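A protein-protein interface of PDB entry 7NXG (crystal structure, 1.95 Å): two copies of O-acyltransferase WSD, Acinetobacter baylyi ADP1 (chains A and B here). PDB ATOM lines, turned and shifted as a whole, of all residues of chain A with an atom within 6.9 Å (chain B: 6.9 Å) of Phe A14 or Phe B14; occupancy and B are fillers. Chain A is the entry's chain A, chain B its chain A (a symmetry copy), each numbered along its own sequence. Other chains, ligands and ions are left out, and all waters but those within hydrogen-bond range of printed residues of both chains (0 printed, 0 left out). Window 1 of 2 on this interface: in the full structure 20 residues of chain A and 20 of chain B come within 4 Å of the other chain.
O of Phe A14 is in hydrogen-bond range of OG of Ser A18 (3.0 Å).
O of Phe B14 lies within hydrogen-bond range of OG of Ser B18 (3.0 Å).
Pro B11 touches Pro A11 (CB to CB, 3.7 Å).
Phe A14 touches Phe B14.
Ser B18 touches Phe A14 (CB to CZ, 3.7 Å).
CB of Ser A18 touches CZ of Phe B14 (3.7 Å).
OG of Ser B18 touches OG of Ser A18, at 3.5 Å.
Phe A14 touches two residues of chain B.
Of chain A, only Phe A14 (3.6 Å) and Ser A18 (3.7 Å) come within 4 Å of Phe B14.
Of the printed residues of chain A, Ser B18 touches Phe A14 and Ser A18.
Of the printed residues of chain A, Pro B11 touches Pro A11 (3.7 Å).
Printed residues of chain B within 4 Å of Pro A11: Pro B11 (3.7 Å).
Of the printed residues of chain B, Ser A18 touches Phe B14 and Ser B18.
Hydrophobic or aromatic side chains of chain B within 4 Å of the printed part of chain A: Pro B11 and Phe B14.
Printed residues of chain A that touch a printed residue of chain B: Pro A11, Phe A14 and Ser A18.
Hydrophobic or aromatic side chains of chain A that line the printed part of chain B: Pro A11 and Phe A14.
Pro B11 touches its own counterpart, Pro A11.
Phe A14 touches its own counterpart, Phe B14.
Phe A14 touches Ser B18, and with the chains exchanged Ser A18 touches Phe B14.
Ser B18 touches its own counterpart, Ser A18.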
ATOM      1  N   LEU A   9      -9.534  -2.241   4.809  1.00  0.00           N
ATOM      2  CA  LEU A   9      -8.733  -1.693   3.716  1.00  0.00           C
ATOM      3  C   LEU A   9      -7.471  -2.528   3.531  1.00  0.00           C
ATOM      4  O   LEU A   9      -6.886  -3.001   4.505  1.00  0.00           O
ATOM      5  CB  LEU A   9      -8.316  -0.256   4.001  1.00  0.00           C
ATOM      6  CG  LEU A   9      -9.383   0.812   4.083  1.00  0.00           C
ATOM      7  CD1 LEU A   9      -8.676   2.158   4.214  1.00  0.00           C
ATOM      8  CD2 LEU A   9     -10.270   0.757   2.875  1.00  0.00           C
ATOM      9  N   HIS A  10      -7.051  -2.708   2.276  1.00  0.00           N
ATOM     10  CA  HIS A  10      -5.733  -3.272   2.004  1.00  0.00           C
ATOM     11  C   HIS A  10      -4.667  -2.204   2.266  1.00  0.00           C
ATOM     12  O   HIS A  10      -4.933  -1.014   2.093  1.00  0.00           O
ATOM     13  CB  HIS A  10      -5.634  -3.740   0.547  1.00  0.00           C
ATOM     14  CG  HIS A  10      -4.472  -4.641   0.285  1.00  0.00           C
ATOM     15  ND1 HIS A  10      -3.211  -4.157  -0.010  1.00  0.00           N
ATOM     16  CD2 HIS A  10      -4.367  -5.992   0.280  1.00  0.00           C
ATOM     17  CE1 HIS A  10      -2.380  -5.174  -0.181  1.00  0.00           C
ATOM     18  NE2 HIS A  10      -3.058  -6.296  -0.008  1.00  0.00           N
ATOM     19  N   PRO A  11      -3.471  -2.592   2.741  1.00  0.00           N
ATOM     20  CA  PRO A  11      -2.393  -1.597   2.906  1.00  0.00           C
ATOM     21  C   PRO A  11      -2.147  -0.733   1.685  1.00  0.00           C
ATOM     22  O   PRO A  11      -1.775   0.441   1.833  1.00  0.00           O
ATOM     23  CB  PRO A  11      -1.169  -2.458   3.216  1.00  0.00           C
ATOM     24  CG  PRO A  11      -1.734  -3.642   3.905  1.00  0.00           C
ATOM     25  CD  PRO A  11      -3.065  -3.907   3.244  1.00  0.00           C
ATOM     26  N   ILE A  12      -2.280  -1.295   0.480  1.00  0.00           N
ATOM     27  CA  ILE A  12      -2.098  -0.506  -0.740  1.00  0.00           C
ATOM     28  C   ILE A  12      -3.157   0.579  -0.818  1.00  0.00           C
ATOM     29  O   ILE A  12      -2.844   1.752  -1.066  1.00  0.00           O
ATOM     30  CB  ILE A  12      -2.120  -1.404  -1.998  1.00  0.00           C
ATOM     31  CG1 ILE A  12      -0.991  -2.441  -1.963  1.00  0.00           C
ATOM     32  CG2 ILE A  12      -2.033  -0.557  -3.271  1.00  0.00           C
ATOM     33  CD1 ILE A  12      -1.213  -3.648  -2.902  1.00  0.00           C
ATOM     34  N   ASP A  13      -4.426   0.202  -0.598  1.00  0.00           N
ATOM     35  CA  ASP A  13      -5.507   1.188  -0.570  1.00  0.00           C
ATOM     36  C   ASP A  13      -5.144   2.331   0.366  1.00  0.00           C
ATOM     37  O   ASP A  13      -5.339   3.503   0.049  1.00  0.00           O
ATOM     38  CB  ASP A  13      -6.829   0.564  -0.091  1.00  0.00           C
ATOM     39  CG  ASP A  13      -7.174  -0.738  -0.778  1.00  0.00           C
ATOM     40  OD1 ASP A  13      -6.683  -0.988  -1.896  1.00  0.00           O
ATOM     41  OD2 ASP A  13      -7.984  -1.501  -0.190  1.00  0.00           O
ATOM     42  N   PHE A  14      -4.668   1.988   1.560  1.00  0.00           N
ATOM     43  CA  PHE A  14      -4.465   2.977   2.609  1.00  0.00           C
ATOM     44  C   PHE A  14      -3.351   3.965   2.259  1.00  0.00           C
ATOM     45  O   PHE A  14      -3.424   5.142   2.650  1.00  0.00           O
ATOM     46  CB  PHE A  14      -4.179   2.244   3.907  1.00  0.00           C
ATOM     47  CG  PHE A  14      -4.076   3.141   5.082  1.00  0.00           C
ATOM     48  CD1 PHE A  14      -5.161   3.895   5.483  1.00  0.00           C
ATOM     49  CD2 PHE A  14      -2.894   3.243   5.781  1.00  0.00           C
ATOM     50  CE1 PHE A  14      -5.077   4.732   6.578  1.00  0.00           C
ATOM     51  CE2 PHE A  14      -2.796   4.082   6.863  1.00  0.00           C
ATOM     52  CZ  PHE A  14      -3.892   4.830   7.266  1.00  0.00           C
ATOM     53  N   ILE A  15      -2.335   3.521   1.507  1.00  0.00           N
ATOM     54  CA  ILE A  15      -1.287   4.438   1.064  1.00  0.00           C
ATOM     55  C   ILE A  15      -1.892   5.606   0.297  1.00  0.00           C
ATOM     56  O   ILE A  15      -1.579   6.770   0.567  1.00  0.00           O
ATOM     57  CB  ILE A  15      -0.232   3.715   0.197  1.00  0.00           C
ATOM     58  CG1 ILE A  15       0.619   2.786   1.053  1.00  0.00           C
ATOM     59  CG2 ILE A  15       0.608   4.727  -0.579  1.00  0.00           C
ATOM     60  CD1 ILE A  15       1.646   1.992   0.258  1.00  0.00           C
ATOM     61  N   PHE A  16      -2.770   5.311  -0.670  1.00  0.00           N
ATOM     62  CA  PHE A  16      -3.256   6.360  -1.572  1.00  0.00           C
ATOM     63  C   PHE A  16      -4.245   7.294  -0.890  1.00  0.00           C
ATOM     64  O   PHE A  16      -4.312   8.482  -1.233  1.00  0.00           O
ATOM     65  CB  PHE A  16      -3.847   5.724  -2.830  1.00  0.00           C
ATOM     66  CG  PHE A  16      -2.801   5.076  -3.694  1.00  0.00           C
ATOM     67  CD1 PHE A  16      -2.024   5.839  -4.565  1.00  0.00           C
ATOM     68  CD2 PHE A  16      -2.556   3.718  -3.613  1.00  0.00           C
ATOM     69  CE1 PHE A  16      -1.033   5.248  -5.342  1.00  0.00           C
ATOM     70  CE2 PHE A  16      -1.562   3.124  -4.398  1.00  0.00           C
ATOM     71  CZ  PHE A  16      -0.803   3.904  -5.262  1.00  0.00           C
ATOM     72  N   LEU A  17      -4.954   6.813   0.130  1.00  0.00           N
ATOM     73  CA  LEU A  17      -5.791   7.715   0.921  1.00  0.00           C
ATOM     74  C   LEU A  17      -4.933   8.588   1.839  1.00  0.00           C
ATOM     75  O   LEU A  17      -5.172   9.793   1.953  1.00  0.00           O
ATOM     76  CB  LEU A  17      -6.810   6.907   1.722  1.00  0.00           C
ATOM     77  CG  LEU A  17      -7.826   6.178   0.828  1.00  0.00           C
ATOM     78  CD1 LEU A  17      -8.605   5.172   1.617  1.00  0.00           C
ATOM     79  CD2 LEU A  17      -8.754   7.157   0.125  1.00  0.00           C
ATOM     80  N   SER A  18      -3.928   8.008   2.500  1.00  0.00           N
ATOM     81  CA  SER A  18      -3.139   8.775   3.473  1.00  0.00           C
ATOM     82  C   SER A  18      -2.292   9.855   2.815  1.00  0.00           C
ATOM     83  O   SER A  18      -1.977  10.858   3.469  1.00  0.00           O
ATOM     84  CB  SER A  18      -2.191   7.877   4.267  1.00  0.00           C
ATOM     85  OG  SER A  18      -2.900   6.921   5.011  1.00  0.00           O
ATOM     86  N   LEU A  19      -1.832   9.634   1.583  1.00  0.00           N
ATOM     87  CA  LEU A  19      -0.949  10.590   0.908  1.00  0.00           C
ATOM     88  C   LEU A  19      -1.698  11.680   0.158  1.00  0.00           C
ATOM     89  O   LEU A  19      -1.065  12.624  -0.342  1.00  0.00           O
ATOM     90  CB  LEU A  19      -0.052   9.855  -0.104  1.00  0.00           C
ATOM     91  CG  LEU A  19       0.923   8.802   0.444  1.00  0.00           C
ATOM     92  CD1 LEU A  19       1.921   8.309  -0.631  1.00  0.00           C
ATOM     93  CD2 LEU A  19       1.637   9.322   1.662  1.00  0.00           C
ATOM     94  N   GLY A  69     -14.396   4.281   8.332  1.00  0.00           N
ATOM     95  CA  GLY A  69     -13.189   4.081   9.128  1.00  0.00           C
ATOM     96  C   GLY A  69     -12.108   3.458   8.266  1.00  0.00           C
ATOM     97  O   GLY A  69     -11.846   3.904   7.152  1.00  0.00           O
ATOM     98  N   LEU A  70     -11.427   2.448   8.792  1.00  0.00           N
ATOM     99  CA  LEU A  70     -10.432   1.726   8.007  1.00  0.00           C
ATOM    100  C   LEU A  70     -11.030   0.504   7.305  1.00  0.00           C
ATOM    101  O   LEU A  70     -10.374  -0.545   7.195  1.00  0.00           O
ATOM    102  CB  LEU A  70      -9.263   1.340   8.902  1.00  0.00           C
ATOM    103  CG  LEU A  70      -8.386   2.513   9.360  1.00  0.00           C
ATOM    104  CD1 LEU A  70      -7.325   2.018  10.328  1.00  0.00           C
ATOM    105  CD2 LEU A  70      -7.711   3.222   8.181  1.00  0.00           C
ATOM    106  N   ALA A 139      -7.086   4.247  -4.516  1.00  0.00           N
ATOM    107  CA  ALA A 139      -7.347   3.359  -3.386  1.00  0.00           C
ATOM    108  C   ALA A 139      -8.234   2.188  -3.788  1.00  0.00           C
ATOM    109  O   ALA A 139      -8.255   1.168  -3.085  1.00  0.00           O
ATOM    110  CB  ALA A 139      -7.983   4.137  -2.229  1.00  0.00           C
ATOM    111  N   LEU B   9       8.719   0.852   5.263  1.00  0.00           N
ATOM    112  CA  LEU B   9       7.845   0.726   6.427  1.00  0.00           C
ATOM    113  C   LEU B   9       6.939  -0.489   6.265  1.00  0.00           C
ATOM    114  O   LEU B   9       6.488  -0.790   5.160  1.00  0.00           O
ATOM    115  CB  LEU B   9       6.965   1.958   6.595  1.00  0.00           C
ATOM    116  CG  LEU B   9       7.616   3.284   6.919  1.00  0.00           C
ATOM    117  CD1 LEU B   9       6.500   4.290   7.186  1.00  0.00           C
ATOM    118  CD2 LEU B   9       8.537   3.139   8.093  1.00  0.00           C
ATOM    119  N   HIS B  10       6.672  -1.188   7.371  1.00  0.00           N
ATOM    120  CA  HIS B  10       5.629  -2.209   7.374  1.00  0.00           C
ATOM    121  C   HIS B  10       4.258  -1.526   7.409  1.00  0.00           C
ATOM    122  O   HIS B  10       4.129  -0.437   7.968  1.00  0.00           O
ATOM    123  CB  HIS B  10       5.770  -3.124   8.597  1.00  0.00           C
ATOM    124  CG  HIS B  10       4.984  -4.390   8.492  1.00  0.00           C
ATOM    125  ND1 HIS B  10       3.653  -4.468   8.856  1.00  0.00           N
ATOM    126  CD2 HIS B  10       5.329  -5.626   8.058  1.00  0.00           C
ATOM    127  CE1 HIS B  10       3.212  -5.699   8.645  1.00  0.00           C
ATOM    128  NE2 HIS B  10       4.210  -6.418   8.161  1.00  0.00           N
ATOM    129  N   PRO B  11       3.231  -2.111   6.769  1.00  0.00           N
ATOM    130  CA  PRO B  11       1.880  -1.527   6.872  1.00  0.00           C
ATOM    131  C   PRO B  11       1.431  -1.231   8.289  1.00  0.00           C
ATOM    132  O   PRO B  11       0.687  -0.262   8.505  1.00  0.00           O
ATOM    133  CB  PRO B  11       0.991  -2.595   6.235  1.00  0.00           C
ATOM    134  CG  PRO B  11       1.873  -3.241   5.236  1.00  0.00           C
ATOM    135  CD  PRO B  11       3.252  -3.252   5.850  1.00  0.00           C
ATOM    136  N   ILE B  12       1.809  -2.073   9.257  1.00  0.00           N
ATOM    137  CA  ILE B  12       1.446  -1.822  10.653  1.00  0.00           C
ATOM    138  C   ILE B  12       2.093  -0.535  11.133  1.00  0.00           C
ATOM    139  O   ILE B  12       1.427   0.325  11.725  1.00  0.00           O
ATOM    140  CB  ILE B  12       1.831  -3.015  11.556  1.00  0.00           C
ATOM    141  CG1 ILE B  12       1.105  -4.296  11.128  1.00  0.00           C
ATOM    142  CG2 ILE B  12       1.542  -2.699  13.026  1.00  0.00           C
ATOM    143  CD1 ILE B  12       1.763  -5.597  11.643  1.00  0.00           C
ATOM    144  N   ASP B  13       3.401  -0.384  10.875  1.00  0.00           N
ATOM    145  CA  ASP B  13       4.096   0.856  11.224  1.00  0.00           C
ATOM    146  C   ASP B  13       3.327   2.053  10.685  1.00  0.00           C
ATOM    147  O   ASP B  13       3.143   3.057  11.370  1.00  0.00           O
ATOM    148  CB  ASP B  13       5.520   0.889  10.645  1.00  0.00           C
ATOM    149  CG  ASP B  13       6.311  -0.375  10.897  1.00  0.00           C
ATOM    150  OD1 ASP B  13       5.992  -1.116  11.847  1.00  0.00           O
ATOM    151  OD2 ASP B  13       7.292  -0.599  10.142  1.00  0.00           O
ATOM    152  N   PHE B  14       2.924   1.974   9.419  1.00  0.00           N
ATOM    153  CA  PHE B  14       2.349   3.123   8.732  1.00  0.00           C
ATOM    154  C   PHE B  14       0.994   3.523   9.318  1.00  0.00           C
ATOM    155  O   PHE B  14       0.655   4.718   9.329  1.00  0.00           O
ATOM    156  CB  PHE B  14       2.249   2.793   7.254  1.00  0.00           C
ATOM    157  CG  PHE B  14       1.792   3.933   6.425  1.00  0.00           C
ATOM    158  CD1 PHE B  14       2.545   5.087   6.347  1.00  0.00           C
ATOM    159  CD2 PHE B  14       0.604   3.859   5.730  1.00  0.00           C
ATOM    160  CE1 PHE B  14       2.130   6.153   5.574  1.00  0.00           C
ATOM    161  CE2 PHE B  14       0.176   4.919   4.970  1.00  0.00           C
ATOM    162  CZ  PHE B  14       0.942   6.072   4.890  1.00  0.00           C
ATOM    163  N   ILE B  15       0.224   2.554   9.830  1.00  0.00           N
ATOM    164  CA  ILE B  15      -1.041   2.884  10.484  1.00  0.00           C
ATOM    165  C   ILE B  15      -0.811   3.875  11.618  1.00  0.00           C
ATOM    166  O   ILE B  15      -1.503   4.893  11.717  1.00  0.00           O
ATOM    167  CB  ILE B  15      -1.750   1.617  11.014  1.00  0.00           C
ATOM    168  CG1 ILE B  15      -2.295   0.787   9.861  1.00  0.00           C
ATOM    169  CG2 ILE B  15      -2.832   1.993  12.025  1.00  0.00           C
ATOM    170  CD1 ILE B  15      -2.959  -0.510  10.301  1.00  0.00           C
ATOM    171  N   PHE B  16       0.167   3.591  12.486  1.00  0.00           N
ATOM    172  CA  PHE B  16       0.332   4.394  13.702  1.00  0.00           C
ATOM    173  C   PHE B  16       0.920   5.766  13.411  1.00  0.00           C
ATOM    174  O   PHE B  16       0.613   6.735  14.120  1.00  0.00           O
ATOM    175  CB  PHE B  16       1.168   3.620  14.721  1.00  0.00           C
ATOM    176  CG  PHE B  16       0.443   2.424  15.273  1.00  0.00           C
ATOM    177  CD1 PHE B  16      -0.492   2.568  16.298  1.00  0.00           C
ATOM    178  CD2 PHE B  16       0.653   1.163  14.748  1.00  0.00           C
ATOM    179  CE1 PHE B  16      -1.190   1.470  16.788  1.00  0.00           C
ATOM    180  CE2 PHE B  16      -0.047   0.057  15.245  1.00  0.00           C
ATOM    181  CZ  PHE B  16      -0.970   0.225  16.269  1.00  0.00           C
ATOM    182  N   LEU B  17       1.691   5.899  12.332  1.00  0.00           N
ATOM    183  CA  LEU B  17       2.139   7.228  11.919  1.00  0.00           C
ATOM    184  C   LEU B  17       0.993   8.017  11.284  1.00  0.00           C
ATOM    185  O   LEU B  17       0.817   9.202  11.575  1.00  0.00           O
ATOM    186  CB  LEU B  17       3.321   7.101  10.960  1.00  0.00           C
ATOM    187  CG  LEU B  17       4.568   6.499  11.629  1.00  0.00           C
ATOM    188  CD1 LEU B  17       5.589   6.114  10.603  1.00  0.00           C
ATOM    189  CD2 LEU B  17       5.161   7.449  12.658  1.00  0.00           C
ATOM    190  N   SER B  18       0.199   7.382  10.417  1.00  0.00           N
ATOM    191  CA  SER B  18      -0.851   8.117   9.699  1.00  0.00           C
ATOM    192  C   SER B  18      -1.967   8.588  10.619  1.00  0.00           C
ATOM    193  O   SER B  18      -2.630   9.586  10.304  1.00  0.00           O
ATOM    194  CB  SER B  18      -1.494   7.262   8.606  1.00  0.00           C
ATOM    195  OG  SER B  18      -0.553   6.883   7.636  1.00  0.00           O
ATOM    196  N   LEU B  19      -2.261   7.847  11.688  1.00  0.00           N
ATOM    197  CA  LEU B  19      -3.369   8.190  12.583  1.00  0.00           C
ATOM    198  C   LEU B  19      -2.978   9.165  13.684  1.00  0.00           C
ATOM    199  O   LEU B  19      -3.857   9.636  14.424  1.00  0.00           O
ATOM    200  CB  LEU B  19      -3.917   6.919  13.255  1.00  0.00           C
ATOM    201  CG  LEU B  19      -4.522   5.838  12.345  1.00  0.00           C
ATOM    202  CD1 LEU B  19      -5.242   4.729  13.148  1.00  0.00           C
ATOM    203  CD2 LEU B  19      -5.433   6.457  11.320  1.00  0.00           C
ATOM    204  N   GLY B  69      10.969   9.372   4.289  1.00  0.00           N
ATOM    205  CA  GLY B  69       9.852   9.053   3.406  1.00  0.00           C
ATOM    206  C   GLY B  69       9.085   7.868   3.962  1.00  0.00           C
ATOM    207  O   GLY B  69       8.753   7.822   5.144  1.00  0.00           O
ATOM    208  N   LEU B  70       8.745   6.915   3.103  1.00  0.00           N
ATOM    209  CA  LEU B  70       8.087   5.697   3.559  1.00  0.00           C
ATOM    210  C   LEU B  70       9.091   4.582   3.864  1.00  0.00           C
ATOM    211  O   LEU B  70       8.822   3.399   3.596  1.00  0.00           O
ATOM    212  CB  LEU B  70       7.061   5.257   2.524  1.00  0.00           C
ATOM    213  CG  LEU B  70       5.824   6.158   2.417  1.00  0.00           C
ATOM    214  CD1 LEU B  70       4.932   5.680   1.285  1.00  0.00           C
ATOM    215  CD2 LEU B  70       5.020   6.189   3.722  1.00  0.00           C
ATOM    216  N   ALA B 139       4.800   2.830  16.023  1.00  0.00           N
ATOM    217  CA  ALA B 139       5.276   2.488  14.685  1.00  0.00           C
ATOM    218  C   ALA B 139       6.518   1.609  14.739  1.00  0.00           C
ATOM    219  O   ALA B 139       6.834   0.935  13.749  1.00  0.00           O
ATOM    220  CB  ALA B 139       5.556   3.759  13.875  1.00  0.00           C
